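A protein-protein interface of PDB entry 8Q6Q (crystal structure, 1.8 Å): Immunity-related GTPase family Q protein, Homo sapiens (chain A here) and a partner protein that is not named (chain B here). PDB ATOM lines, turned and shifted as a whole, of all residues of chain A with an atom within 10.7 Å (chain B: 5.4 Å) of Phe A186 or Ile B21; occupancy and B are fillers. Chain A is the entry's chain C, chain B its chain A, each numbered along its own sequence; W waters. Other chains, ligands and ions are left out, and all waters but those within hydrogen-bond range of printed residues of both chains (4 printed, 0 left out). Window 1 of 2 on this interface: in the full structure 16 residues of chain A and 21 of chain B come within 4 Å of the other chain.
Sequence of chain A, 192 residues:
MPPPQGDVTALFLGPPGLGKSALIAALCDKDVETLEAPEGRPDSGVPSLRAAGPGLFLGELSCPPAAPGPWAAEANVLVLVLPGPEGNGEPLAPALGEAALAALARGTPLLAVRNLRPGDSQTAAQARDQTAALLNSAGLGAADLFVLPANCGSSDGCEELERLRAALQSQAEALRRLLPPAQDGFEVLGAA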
ATOM      1  N   GLN A   5      -6.193  34.416  11.265  1.00  0.00           N
ATOM      2  CA  GLN A   5      -6.917  33.937  12.450  1.00  0.00           C
ATOM      3  C   GLN A   5      -8.224  33.262  12.095  1.00  0.00           C
ATOM      4  O   GLN A   5      -8.936  32.800  12.976  1.00  0.00           O
ATOM      5  CB  GLN A   5      -7.189  35.088  13.432  1.00  0.00           C
ATOM      6  CG  GLN A   5      -7.357  34.650  14.893  1.00  0.00           C
ATOM      7  CD  GLN A   5      -7.608  35.814  15.865  1.00  0.00           C
ATOM      8  OE1 GLN A   5      -7.368  36.983  15.544  1.00  0.00           O
ATOM      9  NE2 GLN A   5      -8.109  35.490  17.057  1.00  0.00           N
ATOM     10  N   GLY A   6      -8.559  33.181  10.807  1.00  0.00           N
ATOM     11  CA  GLY A   6      -9.801  32.534  10.425  1.00  0.00           C
ATOM     12  C   GLY A   6      -9.673  31.022  10.274  1.00  0.00           C
ATOM     13  O   GLY A   6      -8.608  30.448  10.132  1.00  0.00           O
ATOM     14  N   ASP A   7     -10.797  30.319  10.312  1.00  0.00           N
ATOM     15  CA  ASP A   7     -10.783  28.884  10.084  1.00  0.00           C
ATOM     16  C   ASP A   7     -11.382  28.553   8.725  1.00  0.00           C
ATOM     17  O   ASP A   7     -12.401  29.116   8.342  1.00  0.00           O
ATOM     18  CB  ASP A   7     -11.544  28.190  11.210  1.00  0.00           C
ATOM     19  CG  ASP A   7     -10.824  28.344  12.512  1.00  0.00           C
ATOM     20  OD1 ASP A   7      -9.678  27.852  12.561  1.00  0.00           O
ATOM     21  OD2 ASP A   7     -11.324  29.033  13.433  1.00  0.00           O
ATOM     22  N   VAL A   8     -10.740  27.645   8.008  1.00  0.00           N
ATOM     23  CA  VAL A   8     -11.116  27.298   6.646  1.00  0.00           C
ATOM     24  C   VAL A   8     -11.848  25.976   6.658  1.00  0.00           C
ATOM     25  O   VAL A   8     -11.390  25.029   7.310  1.00  0.00           O
ATOM     26  CB  VAL A   8      -9.876  27.174   5.759  1.00  0.00           C
ATOM     27  CG1 VAL A   8     -10.263  26.594   4.432  1.00  0.00           C
ATOM     28  CG2 VAL A   8      -9.203  28.513   5.632  1.00  0.00           C
ATOM     29  N   THR A   9     -12.951  25.889   5.897  1.00  0.00           N
ATOM     30  CA  THR A   9     -13.735  24.668   5.723  1.00  0.00           C
ATOM     31  C   THR A   9     -13.622  24.200   4.278  1.00  0.00           C
ATOM     32  O   THR A   9     -13.941  24.966   3.351  1.00  0.00           O
ATOM     33  CB  THR A   9     -15.197  24.915   6.067  1.00  0.00           C
ATOM     34  OG1 THR A   9     -15.274  25.446   7.401  1.00  0.00           O
ATOM     35  CG2 THR A   9     -16.006  23.633   5.927  1.00  0.00           C
ATOM     36  N   PRO A  47     -23.354  17.749   9.590  1.00  0.00           N
ATOM     37  CA  PRO A  47     -22.001  17.562   9.031  1.00  0.00           C
ATOM     38  C   PRO A  47     -20.908  17.555  10.106  1.00  0.00           C
ATOM     39  O   PRO A  47     -20.796  18.519  10.865  1.00  0.00           O
ATOM     40  CB  PRO A  47     -21.815  18.784   8.137  1.00  0.00           C
ATOM     41  CG  PRO A  47     -22.530  19.860   8.875  1.00  0.00           C
ATOM     42  CD  PRO A  47     -23.701  19.178   9.657  1.00  0.00           C
ATOM     43  N   SER A  48     -20.100  16.505  10.170  1.00  0.00           N
ATOM     44  CA  SER A  48     -19.009  16.426  11.141  1.00  0.00           C
ATOM     45  C   SER A  48     -17.708  16.903  10.499  1.00  0.00           C
ATOM     46  O   SER A  48     -17.288  16.378   9.464  1.00  0.00           O
ATOM     47  CB  SER A  48     -18.859  15.005  11.669  1.00  0.00           C
ATOM     48  OG  SER A  48     -18.520  14.131  10.606  1.00  0.00           O
ATOM     49  N   LEU A  49     -17.060  17.867  11.130  1.00  0.00           N
ATOM     50  CA  LEU A  49     -15.844  18.465  10.589  1.00  0.00           C
ATOM     51  C   LEU A  49     -14.659  17.869  11.320  1.00  0.00           C
ATOM     52  O   LEU A  49     -14.711  17.680  12.544  1.00  0.00           O
ATOM     53  CB  LEU A  49     -15.870  19.983  10.755  1.00  0.00           C
ATOM     54  CG  LEU A  49     -16.903  20.724   9.917  1.00  0.00           C
ATOM     55  CD1 LEU A  49     -16.830  22.221  10.127  1.00  0.00           C
ATOM     56  CD2 LEU A  49     -16.756  20.409   8.382  1.00  0.00           C
ATOM     57  N   ARG A  50     -13.601  17.541  10.578  1.00  0.00           N
ATOM     58  CA  ARG A  50     -12.396  17.004  11.185  1.00  0.00           C
ATOM     59  C   ARG A  50     -11.227  17.938  10.888  1.00  0.00           C
ATOM     60  O   ARG A  50     -11.102  18.463   9.772  1.00  0.00           O
ATOM     61  CB  ARG A  50     -12.120  15.582  10.691  1.00  0.00           C
ATOM     62  N   PHE A  57     -10.652  22.637   8.475  1.00  0.00           N
ATOM     63  CA  PHE A  57     -11.582  21.575   8.854  1.00  0.00           C
ATOM     64  C   PHE A  57     -12.074  20.948   7.564  1.00  0.00           C
ATOM     65  O   PHE A  57     -12.279  21.660   6.573  1.00  0.00           O
ATOM     66  CB  PHE A  57     -12.746  22.123   9.633  1.00  0.00           C
ATOM     67  CG  PHE A  57     -12.362  22.712  10.954  1.00  0.00           C
ATOM     68  CD1 PHE A  57     -12.210  21.900  12.057  1.00  0.00           C
ATOM     69  CD2 PHE A  57     -12.147  24.062  11.088  1.00  0.00           C
ATOM     70  CE1 PHE A  57     -11.856  22.429  13.308  1.00  0.00           C
ATOM     71  CE2 PHE A  57     -11.799  24.596  12.315  1.00  0.00           C
ATOM     72  CZ  PHE A  57     -11.641  23.795  13.406  1.00  0.00           C
ATOM     73  N   PRO A 180     -13.116  35.202   8.996  1.00  0.00           N
ATOM     74  CA  PRO A 180     -13.134  35.386  10.452  1.00  0.00           C
ATOM     75  C   PRO A 180     -12.864  34.094  11.208  1.00  0.00           C
ATOM     76  O   PRO A 180     -13.082  32.980  10.700  1.00  0.00           O
ATOM     77  CB  PRO A 180     -14.560  35.873  10.704  1.00  0.00           C
ATOM     78  CG  PRO A 180     -15.350  35.160   9.623  1.00  0.00           C
ATOM     79  CD  PRO A 180     -14.456  35.245   8.397  1.00  0.00           C
ATOM     80  N   PRO A 181     -12.425  34.194  12.458  1.00  0.00           N
ATOM     81  CA  PRO A 181     -12.403  33.004  13.317  1.00  0.00           C
ATOM     82  C   PRO A 181     -13.802  32.430  13.513  1.00  0.00           C
ATOM     83  O   PRO A 181     -14.820  33.108  13.348  1.00  0.00           O
ATOM     84  CB  PRO A 181     -11.800  33.514  14.627  1.00  0.00           C
ATOM     85  CG  PRO A 181     -11.957  35.010  14.565  1.00  0.00           C
ATOM     86  CD  PRO A 181     -11.873  35.388  13.124  1.00  0.00           C
ATOM     87  N   ALA A 182     -13.846  31.135  13.841  1.00  0.00           N
ATOM     88  CA  ALA A 182     -15.139  30.477  14.020  1.00  0.00           C
ATOM     89  C   ALA A 182     -15.964  31.140  15.129  1.00  0.00           C
ATOM     90  O   ALA A 182     -17.187  31.233  15.003  1.00  0.00           O
ATOM     91  CB  ALA A 182     -14.952  28.985  14.318  1.00  0.00           C
ATOM     92  N   GLN A 183     -15.306  31.651  16.187  1.00  0.00           N
ATOM     93  CA  GLN A 183     -15.955  32.329  17.320  1.00  0.00           C
ATOM     94  C   GLN A 183     -16.570  33.648  16.911  1.00  0.00           C
ATOM     95  O   GLN A 183     -17.141  34.339  17.765  1.00  0.00           O
ATOM     96  CB  GLN A 183     -14.949  32.667  18.419  1.00  0.00           C
ATOM     97  CG  GLN A 183     -13.955  31.620  18.695  1.00  0.00           C
ATOM     98  CD  GLN A 183     -12.747  31.832  17.784  1.00  0.00           C
ATOM     99  OE1 GLN A 183     -12.821  31.536  16.601  1.00  0.00           O
ATOM    100  NE2 GLN A 183     -11.652  32.371  18.320  1.00  0.00           N
ATOM    101  N   ASP A 184     -16.356  34.071  15.664  1.00  0.00           N
ATOM    102  CA  ASP A 184     -16.835  35.371  15.239  1.00  0.00           C
ATOM    103  C   ASP A 184     -18.289  35.550  15.594  1.00  0.00           C
ATOM    104  O   ASP A 184     -19.156  34.787  15.148  1.00  0.00           O
ATOM    105  CB  ASP A 184     -16.641  35.570  13.733  1.00  0.00           C
ATOM    106  CG  ASP A 184     -16.980  36.999  13.304  1.00  0.00           C
ATOM    107  OD1 ASP A 184     -16.642  37.943  14.069  1.00  0.00           O
ATOM    108  OD2 ASP A 184     -17.587  37.171  12.217  1.00  0.00           O
ATOM    109  N   GLY A 185     -18.547  36.556  16.409  1.00  0.00           N
ATOM    110  CA  GLY A 185     -19.883  36.904  16.762  1.00  0.00           C
ATOM    111  C   GLY A 185     -20.419  36.170  17.970  1.00  0.00           C
ATOM    112  O   GLY A 185     -21.440  36.585  18.519  1.00  0.00           O
ATOM    113  N   PHE A 186     -19.771  35.092  18.398  1.00  0.00           N
ATOM    114  CA  PHE A 186     -20.184  34.405  19.623  1.00  0.00           C
ATOM    115  C   PHE A 186     -19.730  35.184  20.851  1.00  0.00           C
ATOM    116  O   PHE A 186     -18.575  35.606  20.925  1.00  0.00           O
ATOM    117  CB  PHE A 186     -19.548  33.024  19.683  1.00  0.00           C
ATOM    118  CG  PHE A 186     -20.131  32.004  18.749  1.00  0.00           C
ATOM    119  CD1 PHE A 186     -21.302  31.356  19.058  1.00  0.00           C
ATOM    120  CD2 PHE A 186     -19.528  31.746  17.520  1.00  0.00           C
ATOM    121  CE1 PHE A 186     -21.821  30.405  18.213  1.00  0.00           C
ATOM    122  CE2 PHE A 186     -20.067  30.803  16.645  1.00  0.00           C
ATOM    123  CZ  PHE A 186     -21.233  30.127  17.008  1.00  0.00           C
ATOM    124  N   GLU A 187     -20.618  35.345  21.831  1.00  0.00           N
ATOM    125  CA  GLU A 187     -20.181  35.730  23.174  1.00  0.00           C
ATOM    126  C   GLU A 187     -19.610  34.502  23.874  1.00  0.00           C
ATOM    127  O   GLU A 187     -20.364  33.605  24.279  1.00  0.00           O
ATOM    128  CB  GLU A 187     -21.330  36.321  23.988  1.00  0.00           C
ATOM    129  CG  GLU A 187     -21.659  37.739  23.623  1.00  0.00           C
ATOM    130  CD  GLU A 187     -20.773  38.746  24.367  1.00  0.00           C
ATOM    131  OE1 GLU A 187     -20.512  38.535  25.582  1.00  0.00           O
ATOM    132  OE2 GLU A 187     -20.323  39.725  23.731  1.00  0.00           O
ATOM    133  N   VAL A 188     -18.285  34.472  24.042  1.00  0.00           N
ATOM    134  CA  VAL A 188     -17.591  33.360  24.700  1.00  0.00           C
ATOM    135  C   VAL A 188     -17.617  33.587  26.206  1.00  0.00           C
ATOM    136  O   VAL A 188     -16.821  34.355  26.731  1.00  0.00           O
ATOM    137  CB  VAL A 188     -16.157  33.222  24.191  1.00  0.00           C
ATOM    138  CG1 VAL A 188     -15.552  31.942  24.721  1.00  0.00           C
ATOM    139  CG2 VAL A 188     -16.164  33.218  22.682  1.00  0.00           C
ATOM    140  N   LEU A 189     -18.505  32.876  26.905  1.00  0.00           N
ATOM    141  CA  LEU A 189     -18.600  32.935  28.354  1.00  0.00           C
ATOM    142  C   LEU A 189     -17.433  32.198  29.021  1.00  0.00           C
ATOM    143  O   LEU A 189     -17.101  31.071  28.637  1.00  0.00           O
ATOM    144  CB  LEU A 189     -19.930  32.333  28.811  1.00  0.00           C
ATOM    145  CG  LEU A 189     -21.149  32.914  28.091  1.00  0.00           C
ATOM    146  CD1 LEU A 189     -22.484  32.329  28.572  1.00  0.00           C
ATOM    147  CD2 LEU A 189     -21.128  34.415  28.294  1.00  0.00           C
ATOM    148  N   VAL B  16     -22.646  24.410   9.168  1.00  0.00           N
ATOM    149  CA  VAL B  16     -21.192  24.537   9.115  1.00  0.00           C
ATOM    150  C   VAL B  16     -20.707  25.383  10.289  1.00  0.00           C
ATOM    151  O   VAL B  16     -19.676  25.082  10.912  1.00  0.00           O
ATOM    152  CB  VAL B  16     -20.737  25.122   7.761  1.00  0.00           C
ATOM    153  CG1 VAL B  16     -19.282  25.520   7.788  1.00  0.00           C
ATOM    154  CG2 VAL B  16     -21.085  24.131   6.570  1.00  0.00           C
ATOM    155  N   GLU B  17     -21.468  26.429  10.635  1.00  0.00           N
ATOM    156  CA  GLU B  17     -21.100  27.286  11.760  1.00  0.00           C
ATOM    157  C   GLU B  17     -21.004  26.503  13.056  1.00  0.00           C
ATOM    158  O   GLU B  17     -20.004  26.606  13.783  1.00  0.00           O
ATOM    159  CB  GLU B  17     -22.091  28.435  11.901  1.00  0.00           C
ATOM    160  CG  GLU B  17     -21.569  29.551  12.764  1.00  0.00           C
ATOM    161  CD  GLU B  17     -22.467  30.772  12.762  1.00  0.00           C
ATOM    162  OE1 GLU B  17     -23.049  31.118  11.698  1.00  0.00           O
ATOM    163  OE2 GLU B  17     -22.614  31.362  13.845  1.00  0.00           O
ATOM    164  N   SER B  18     -22.043  25.730  13.381  1.00  0.00           N
ATOM    165  CA  SER B  18     -22.018  25.010  14.657  1.00  0.00           C
ATOM    166  C   SER B  18     -20.983  23.903  14.615  1.00  0.00           C
ATOM    167  O   SER B  18     -20.262  23.666  15.598  1.00  0.00           O
ATOM    168  CB  SER B  18     -23.409  24.424  14.990  1.00  0.00           C
ATOM    169  OG  SER B  18     -23.742  23.466  13.996  1.00  0.00           O
ATOM    170  N   ALA B  19     -20.865  23.244  13.462  1.00  0.00           N
ATOM    171  CA  ALA B  19     -19.887  22.181  13.328  1.00  0.00           C
ATOM    172  C   ALA B  19     -18.480  22.713  13.557  1.00  0.00           C
ATOM    173  O   ALA B  19     -17.654  22.060  14.206  1.00  0.00           O
ATOM    174  CB  ALA B  19     -20.020  21.524  11.948  1.00  0.00           C
ATOM    175  N   LYS B  20     -18.162  23.886  12.975  1.00  0.00           N
ATOM    176  CA  LYS B  20     -16.840  24.454  13.163  1.00  0.00           C
ATOM    177  C   LYS B  20     -16.613  24.784  14.627  1.00  0.00           C
ATOM    178  O   LYS B  20     -15.549  24.505  15.180  1.00  0.00           O
ATOM    179  CB  LYS B  20     -16.664  25.725  12.327  1.00  0.00           C
ATOM    180  CG  LYS B  20     -16.324  25.493  10.882  1.00  0.00           C
ATOM    181  CD  LYS B  20     -15.722  26.721  10.212  1.00  0.00           C
ATOM    182  CE  LYS B  20     -16.759  27.821   9.994  1.00  0.00           C
ATOM    183  NZ  LYS B  20     -15.954  29.084   9.636  1.00  0.00           N
ATOM    184  N   ILE B  21     -17.595  25.423  15.259  1.00  0.00           N
ATOM    185  CA  ILE B  21     -17.402  25.829  16.649  1.00  0.00           C
ATOM    186  C   ILE B  21     -17.404  24.609  17.599  1.00  0.00           C
ATOM    187  O   ILE B  21     -16.670  24.586  18.602  1.00  0.00           O
ATOM    188  CB  ILE B  21     -18.454  26.889  17.022  1.00  0.00           C
ATOM    189  CG1 ILE B  21     -17.830  27.939  17.954  1.00  0.00           C
ATOM    190  CG2 ILE B  21     -19.536  26.271  17.750  1.00  0.00           C
ATOM    191  CD1 ILE B  21     -16.645  28.655  17.342  1.00  0.00           C
ATOM    192  N   ARG B  22     -18.140  23.550  17.260  1.00  0.00           N
ATOM    193  CA  ARG B  22     -18.093  22.321  18.063  1.00  0.00           C
ATOM    194  C   ARG B  22     -16.755  21.605  17.913  1.00  0.00           C
ATOM    195  O   ARG B  22     -16.239  21.023  18.884  1.00  0.00           O
ATOM    196  CB  ARG B  22     -19.235  21.373  17.662  1.00  0.00           C
ATOM    197  CG  ARG B  22     -20.633  21.691  18.224  1.00  0.00           C
ATOM    198  CD  ARG B  22     -20.675  21.601  19.753  1.00  0.00           C
ATOM    199  NE  ARG B  22     -20.582  20.203  20.140  1.00  0.00           N
ATOM    200  CZ  ARG B  22     -20.261  19.778  21.352  1.00  0.00           C
ATOM    201  NH1 ARG B  22     -20.060  20.625  22.348  1.00  0.00           N
ATOM    202  NH2 ARG B  22     -20.193  18.469  21.585  1.00  0.00           N
ATOM    203  N   ALA B  23     -16.199  21.580  16.693  1.00  0.00           N
ATOM    204  CA  ALA B  23     -14.908  20.937  16.513  1.00  0.00           C
ATOM    205  C   ALA B  23     -13.831  21.730  17.230  1.00  0.00           C
ATOM    206  O   ALA B  23     -12.933  21.159  17.851  1.00  0.00           O
ATOM    207  CB  ALA B  23     -14.567  20.805  15.020  1.00  0.00           C
ATOM    208  N   LYS B  24     -13.925  23.053  17.160  1.00  0.00           N
ATOM    209  CA  LYS B  24     -12.888  23.910  17.713  1.00  0.00           C
ATOM    210  C   LYS B  24     -12.998  24.055  19.238  1.00  0.00           C
ATOM    211  O   LYS B  24     -11.983  24.126  19.922  1.00  0.00           O
ATOM    212  CB  LYS B  24     -12.950  25.258  16.991  1.00  0.00           C
ATOM    213  CG  LYS B  24     -11.740  26.074  17.140  1.00  0.00           C
ATOM    214  CD  LYS B  24     -11.922  27.425  16.538  1.00  0.00           C
ATOM    215  CE  LYS B  24     -10.596  28.136  16.514  1.00  0.00           C
ATOM    216  NZ  LYS B  24     -10.731  29.488  15.913  1.00  0.00           N
ATOM    217  N   TYR B  25     -14.205  24.069  19.809  1.00  0.00           N
ATOM    218  CA  TYR B  25     -14.408  24.202  21.255  1.00  0.00           C
ATOM    219  C   TYR B  25     -15.234  23.019  21.739  1.00  0.00           C
ATOM    220  O   TYR B  25     -16.454  23.148  21.876  1.00  0.00           O
ATOM    221  CB  TYR B  25     -15.118  25.511  21.592  1.00  0.00           C
ATOM    222  CG  TYR B  25     -14.333  26.720  21.213  1.00  0.00           C
ATOM    223  CD1 TYR B  25     -14.626  27.458  20.061  1.00  0.00           C
ATOM    224  CD2 TYR B  25     -13.332  27.172  22.047  1.00  0.00           C
ATOM    225  CE1 TYR B  25     -13.893  28.583  19.729  1.00  0.00           C
ATOM    226  CE2 TYR B  25     -12.604  28.309  21.735  1.00  0.00           C
ATOM    227  CZ  TYR B  25     -12.888  29.011  20.574  1.00  0.00           C
ATOM    228  OH  TYR B  25     -12.109  30.126  20.295  1.00  0.00           O
ATOM    229  N   PRO B  26     -14.627  21.844  21.931  1.00  0.00           N
ATOM    230  CA  PRO B  26     -15.442  20.644  22.197  1.00  0.00           C
ATOM    231  C   PRO B  26     -16.077  20.634  23.586  1.00  0.00           C
ATOM    232  O   PRO B  26     -17.030  19.870  23.796  1.00  0.00           O
ATOM    233  CB  PRO B  26     -14.462  19.478  22.021  1.00  0.00           C
ATOM    234  CG  PRO B  26     -13.202  20.047  21.465  1.00  0.00           C
ATOM    235  CD  PRO B  26     -13.236  21.540  21.547  1.00  0.00           C
ATOM    236  N   PRO B  30     -22.827  25.870  21.493  1.00  0.00           N
ATOM    237  CA  PRO B  30     -23.308  27.111  20.861  1.00  0.00           C
ATOM    238  C   PRO B  30     -24.808  27.278  21.107  1.00  0.00           C
ATOM    239  O   PRO B  30     -25.576  26.325  20.880  1.00  0.00           O
ATOM    240  CB  PRO B  30     -23.003  26.875  19.371  1.00  0.00           C
ATOM    241  CG  PRO B  30     -23.226  25.355  19.220  1.00  0.00           C
ATOM    242  CD  PRO B  30     -22.719  24.751  20.531  1.00  0.00           C
ATOM    243  N   VAL B  31     -25.232  28.461  21.566  1.00  0.00           N
ATOM    244  CA  VAL B  31     -26.616  28.690  21.979  1.00  0.00           C
ATOM    245  C   VAL B  31     -27.133  29.995  21.391  1.00  0.00           C
ATOM    246  O   VAL B  31     -26.453  31.029  21.425  1.00  0.00           O
ATOM    247  CB  VAL B  31     -26.722  28.718  23.524  1.00  0.00           C
ATOM    248  CG1 VAL B  31     -28.201  28.870  23.978  1.00  0.00           C
ATOM    249  CG2 VAL B  31     -26.061  27.471  24.122  1.00  0.00           C
ATOM    250  N   LYS B  46     -27.221  40.641  22.924  1.00  0.00           N
ATOM    251  CA  LYS B  46     -26.536  39.646  22.108  1.00  0.00           C
ATOM    252  C   LYS B  46     -27.319  38.334  22.116  1.00  0.00           C
ATOM    253  O   LYS B  46     -27.816  37.914  23.158  1.00  0.00           O
ATOM    254  CB  LYS B  46     -25.100  39.441  22.599  1.00  0.00           C
ATOM    255  CG  LYS B  46     -24.168  40.570  22.128  1.00  0.00           C
ATOM    256  CD  LYS B  46     -22.684  40.193  22.182  1.00  0.00           C
ATOM    257  CE  LYS B  46     -22.094  40.010  20.767  1.00  0.00           C
ATOM    258  NZ  LYS B  46     -20.860  39.150  20.673  1.00  0.00           N
ATOM    259  N   LYS B  48     -26.049  35.294  20.531  1.00  0.00           N
ATOM    260  CA  LYS B  48     -25.292  34.101  20.164  1.00  0.00           C
ATOM    261  C   LYS B  48     -24.195  33.889  21.190  1.00  0.00           C
ATOM    262  O   LYS B  48     -23.354  34.764  21.395  1.00  0.00           O
ATOM    263  CB  LYS B  48     -24.697  34.219  18.755  1.00  0.00           C
ATOM    264  CG  LYS B  48     -24.612  32.914  17.991  1.00  0.00           C
ATOM    265  CD  LYS B  48     -23.402  32.815  17.049  1.00  0.00           C
ATOM    266  CE  LYS B  48     -23.163  34.092  16.261  1.00  0.00           C
ATOM    267  NZ  LYS B  48     -22.593  33.857  14.859  1.00  0.00           N
ATOM    268  N   TYR B  49     -24.196  32.725  21.812  1.00  0.00           N
ATOM    269  CA  TYR B  49     -23.357  32.456  22.970  1.00  0.00           C
ATOM    270  C   TYR B  49     -22.590  31.163  22.778  1.00  0.00           C
ATOM    271  O   TYR B  49     -23.093  30.207  22.187  1.00  0.00           O
ATOM    272  CB  TYR B  49     -24.213  32.351  24.291  1.00  0.00           C
ATOM    273  CG  TYR B  49     -24.836  33.658  24.642  1.00  0.00           C
ATOM    274  CD1 TYR B  49     -26.038  34.055  24.060  1.00  0.00           C
ATOM    275  CD2 TYR B  49     -24.162  34.559  25.482  1.00  0.00           C
ATOM    276  CE1 TYR B  49     -26.598  35.274  24.335  1.00  0.00           C
ATOM    277  CE2 TYR B  49     -24.723  35.783  25.782  1.00  0.00           C
ATOM    278  CZ  TYR B  49     -25.949  36.135  25.204  1.00  0.00           C
ATOM    279  OH  TYR B  49     -26.502  37.358  25.486  1.00  0.00           O
ATOM    280  N   LEU B  50     -21.399  31.121  23.347  1.00  0.00           N
ATOM    281  CA  LEU B  50     -20.601  29.906  23.444  1.00  0.00           C
ATOM    282  C   LEU B  50     -20.484  29.601  24.925  1.00  0.00           C
ATOM    283  O   LEU B  50     -19.757  30.299  25.643  1.00  0.00           O
ATOM    284  CB  LEU B  50     -19.207  30.110  22.827  1.00  0.00           C
ATOM    285  CG  LEU B  50     -18.521  28.853  22.350  1.00  0.00           C
ATOM    286  CD1 LEU B  50     -19.498  28.063  21.483  1.00  0.00           C
ATOM    287  CD2 LEU B  50     -17.227  29.227  21.580  1.00  0.00           C
ATOM    288  N   PHE B 104     -27.160  24.098  16.691  1.00  0.00           N
ATOM    289  CA  PHE B 104     -27.334  25.114  17.716  1.00  0.00           C
ATOM    290  C   PHE B 104     -28.404  24.655  18.707  1.00  0.00           C
ATOM    291  O   PHE B 104     -29.306  23.880  18.356  1.00  0.00           O
ATOM    292  CB  PHE B 104     -27.761  26.448  17.104  1.00  0.00           C
ATOM    293  CG  PHE B 104     -26.630  27.219  16.506  1.00  0.00           C
ATOM    294  CD1 PHE B 104     -25.865  28.090  17.271  1.00  0.00           C
ATOM    295  CD2 PHE B 104     -26.277  26.988  15.175  1.00  0.00           C
ATOM    296  CE1 PHE B 104     -24.772  28.784  16.659  1.00  0.00           C
ATOM    297  CE2 PHE B 104     -25.219  27.678  14.550  1.00  0.00           C
ATOM    298  CZ  PHE B 104     -24.454  28.559  15.302  1.00  0.00           C
HETATM  299  O   HOH W   1     -14.537  31.074   8.721  1.00  0.00           O
HETATM  300  O   HOH W   2     -15.849  28.227   7.110  1.00  0.00           O
HETATM  301  O   HOH W   3     -18.209  28.784  13.342  1.00  0.00           O
HETATM  302  O   HOH W   4     -18.027  19.108  14.082  1.00  0.00           O
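N of Leu B50 is in hydrogen-bond range of O of Glu A187, 2.8 Å away. The side-chain amino group (NZ) of Lys B46 sits at hydrogen-bond distance from the backbone carbonyl oxygen (O) of Gly A185 (3.4 Å). The side-chain amino group (NZ) of Lys B24 lies within hydrogen-bond range of the side-chain amide oxygen (OE1) of Gln A183, at 3.0 Å. OE2 of Glu A187 lies within salt-bridge range of NZ of Lys B46 (3.2 Å). The backbone carbonyl oxygen (O) of Leu B50 sits at hydrogen-bond distance from the backbone NH (N) of Leu A189 (3.1 Å). OD2 of Asp A7 lies within salt-bridge range of NZ of Lys B24 (2.6 Å). The backbone carbonyl oxygen (O) of Lys B48 is in hydrogen-bond range of the backbone NH (N) of Glu A187. The side-chain hydroxyl of Tyr B25 sits close to the side-chain amide nitrogen of Gln A183.
The backbone carbonyl oxygen (O) of Tyr B49 lies within hydrogen-bond range of the backbone NH (N) of Val B31, at 2.8 Å. The side-chain hydroxyl of Tyr B49 sits at hydrogen-bond distance from the backbone carbonyl oxygen of Lys B46, at 2.7 Å. O of Val A8 is in hydrogen-bond range of N of Phe A57, at 2.8 Å.
Among the printed residues, pairs that only touch across the chains: Phe A186 with Lys B48 (3.1 Å), Thr A9 with Lys B20 (3.1 Å), Pro A47 with Ala B19 (3.3 Å), Leu A49 with Lys B20 (3.4 Å), Ala A182 with Ile B21 (3.4 Å), Glu A187 with Tyr B49 (3.5 Å), Gln A183 with Ile B21 (3.5 Å), Asp A184 with Lys B48 (3.6 Å), Phe A57 with Ala B23 (3.6 Å), Phe A186 with Glu B17 (3.7 Å), Phe A186 with Phe B104 (3.7 Å), Leu A49 with Ala B19 (3.7 Å), Gly A185 with Lys B48 (3.8 Å), Asp A7 with Lys B20 (3.8 Å), Phe A186 with Tyr B49 (3.8 Å), Phe A186 with Ile B21 (3.9 Å), Val A188 with Leu B50 (3.9 Å), Phe A186 with Pro B30 (3.9 Å) and Leu A49 with Ala B23 (3.99 Å).
Arg A50 touches none of the printed residues of chain B. Printed residues of chain B within 4 Å of Gln A183: Ile B21, Lys B24 and Tyr B25. Of the printed residues of chain B, Asp A184 touches Lys B48. No residue of chain A comes within 4 Å of Ser B18. Ile B21 touches just these residues of chain A: Ala A182 (3.4 Å), Gln A183 (3.5 Å) and Phe A186 (3.9 Å). Printed residues of chain A within 4 Å of Ala B23: Leu A49 (3.99 Å) and Phe A57 (3.6 Å). Pro B30 touches one residue of chain A. Of chain A, only Glu A187 (2.8 Å), Val A188 (3.9 Å) and Leu A189 (3.1 Å) come within 4 Å of Leu B50. The nearest residue of chain A that does not touch Ile B21 is Asp A184 (5.7 Å). The nearest printed residue of chain B that does not touch Thr A9 is Val B16 (4.03 Å).
Of the 18 printed residues of chain B, 13 touch a printed residue of chain A. Hydrophobic or aromatic side chains of chain B that line the printed part of chain A: Ala B19, Ile B21, Ala B23, Tyr B25, Pro B30, Tyr B49, Leu B50 and Phe B104. Among the printed residues, 27 pairs touch across the chains.
Water W1 lies within hydrogen-bond range of NZ of Lys B20, O of Asp A7 and O of Pro A180. Water W2 bridges NZ of Lys B20 and OG1 of Thr A9. Water W4 bridges the backbone carbonyl oxygen (O) of Ala B19 (3.0 Å) and the backbone NH (N) of Leu A49 (3.3 Å).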
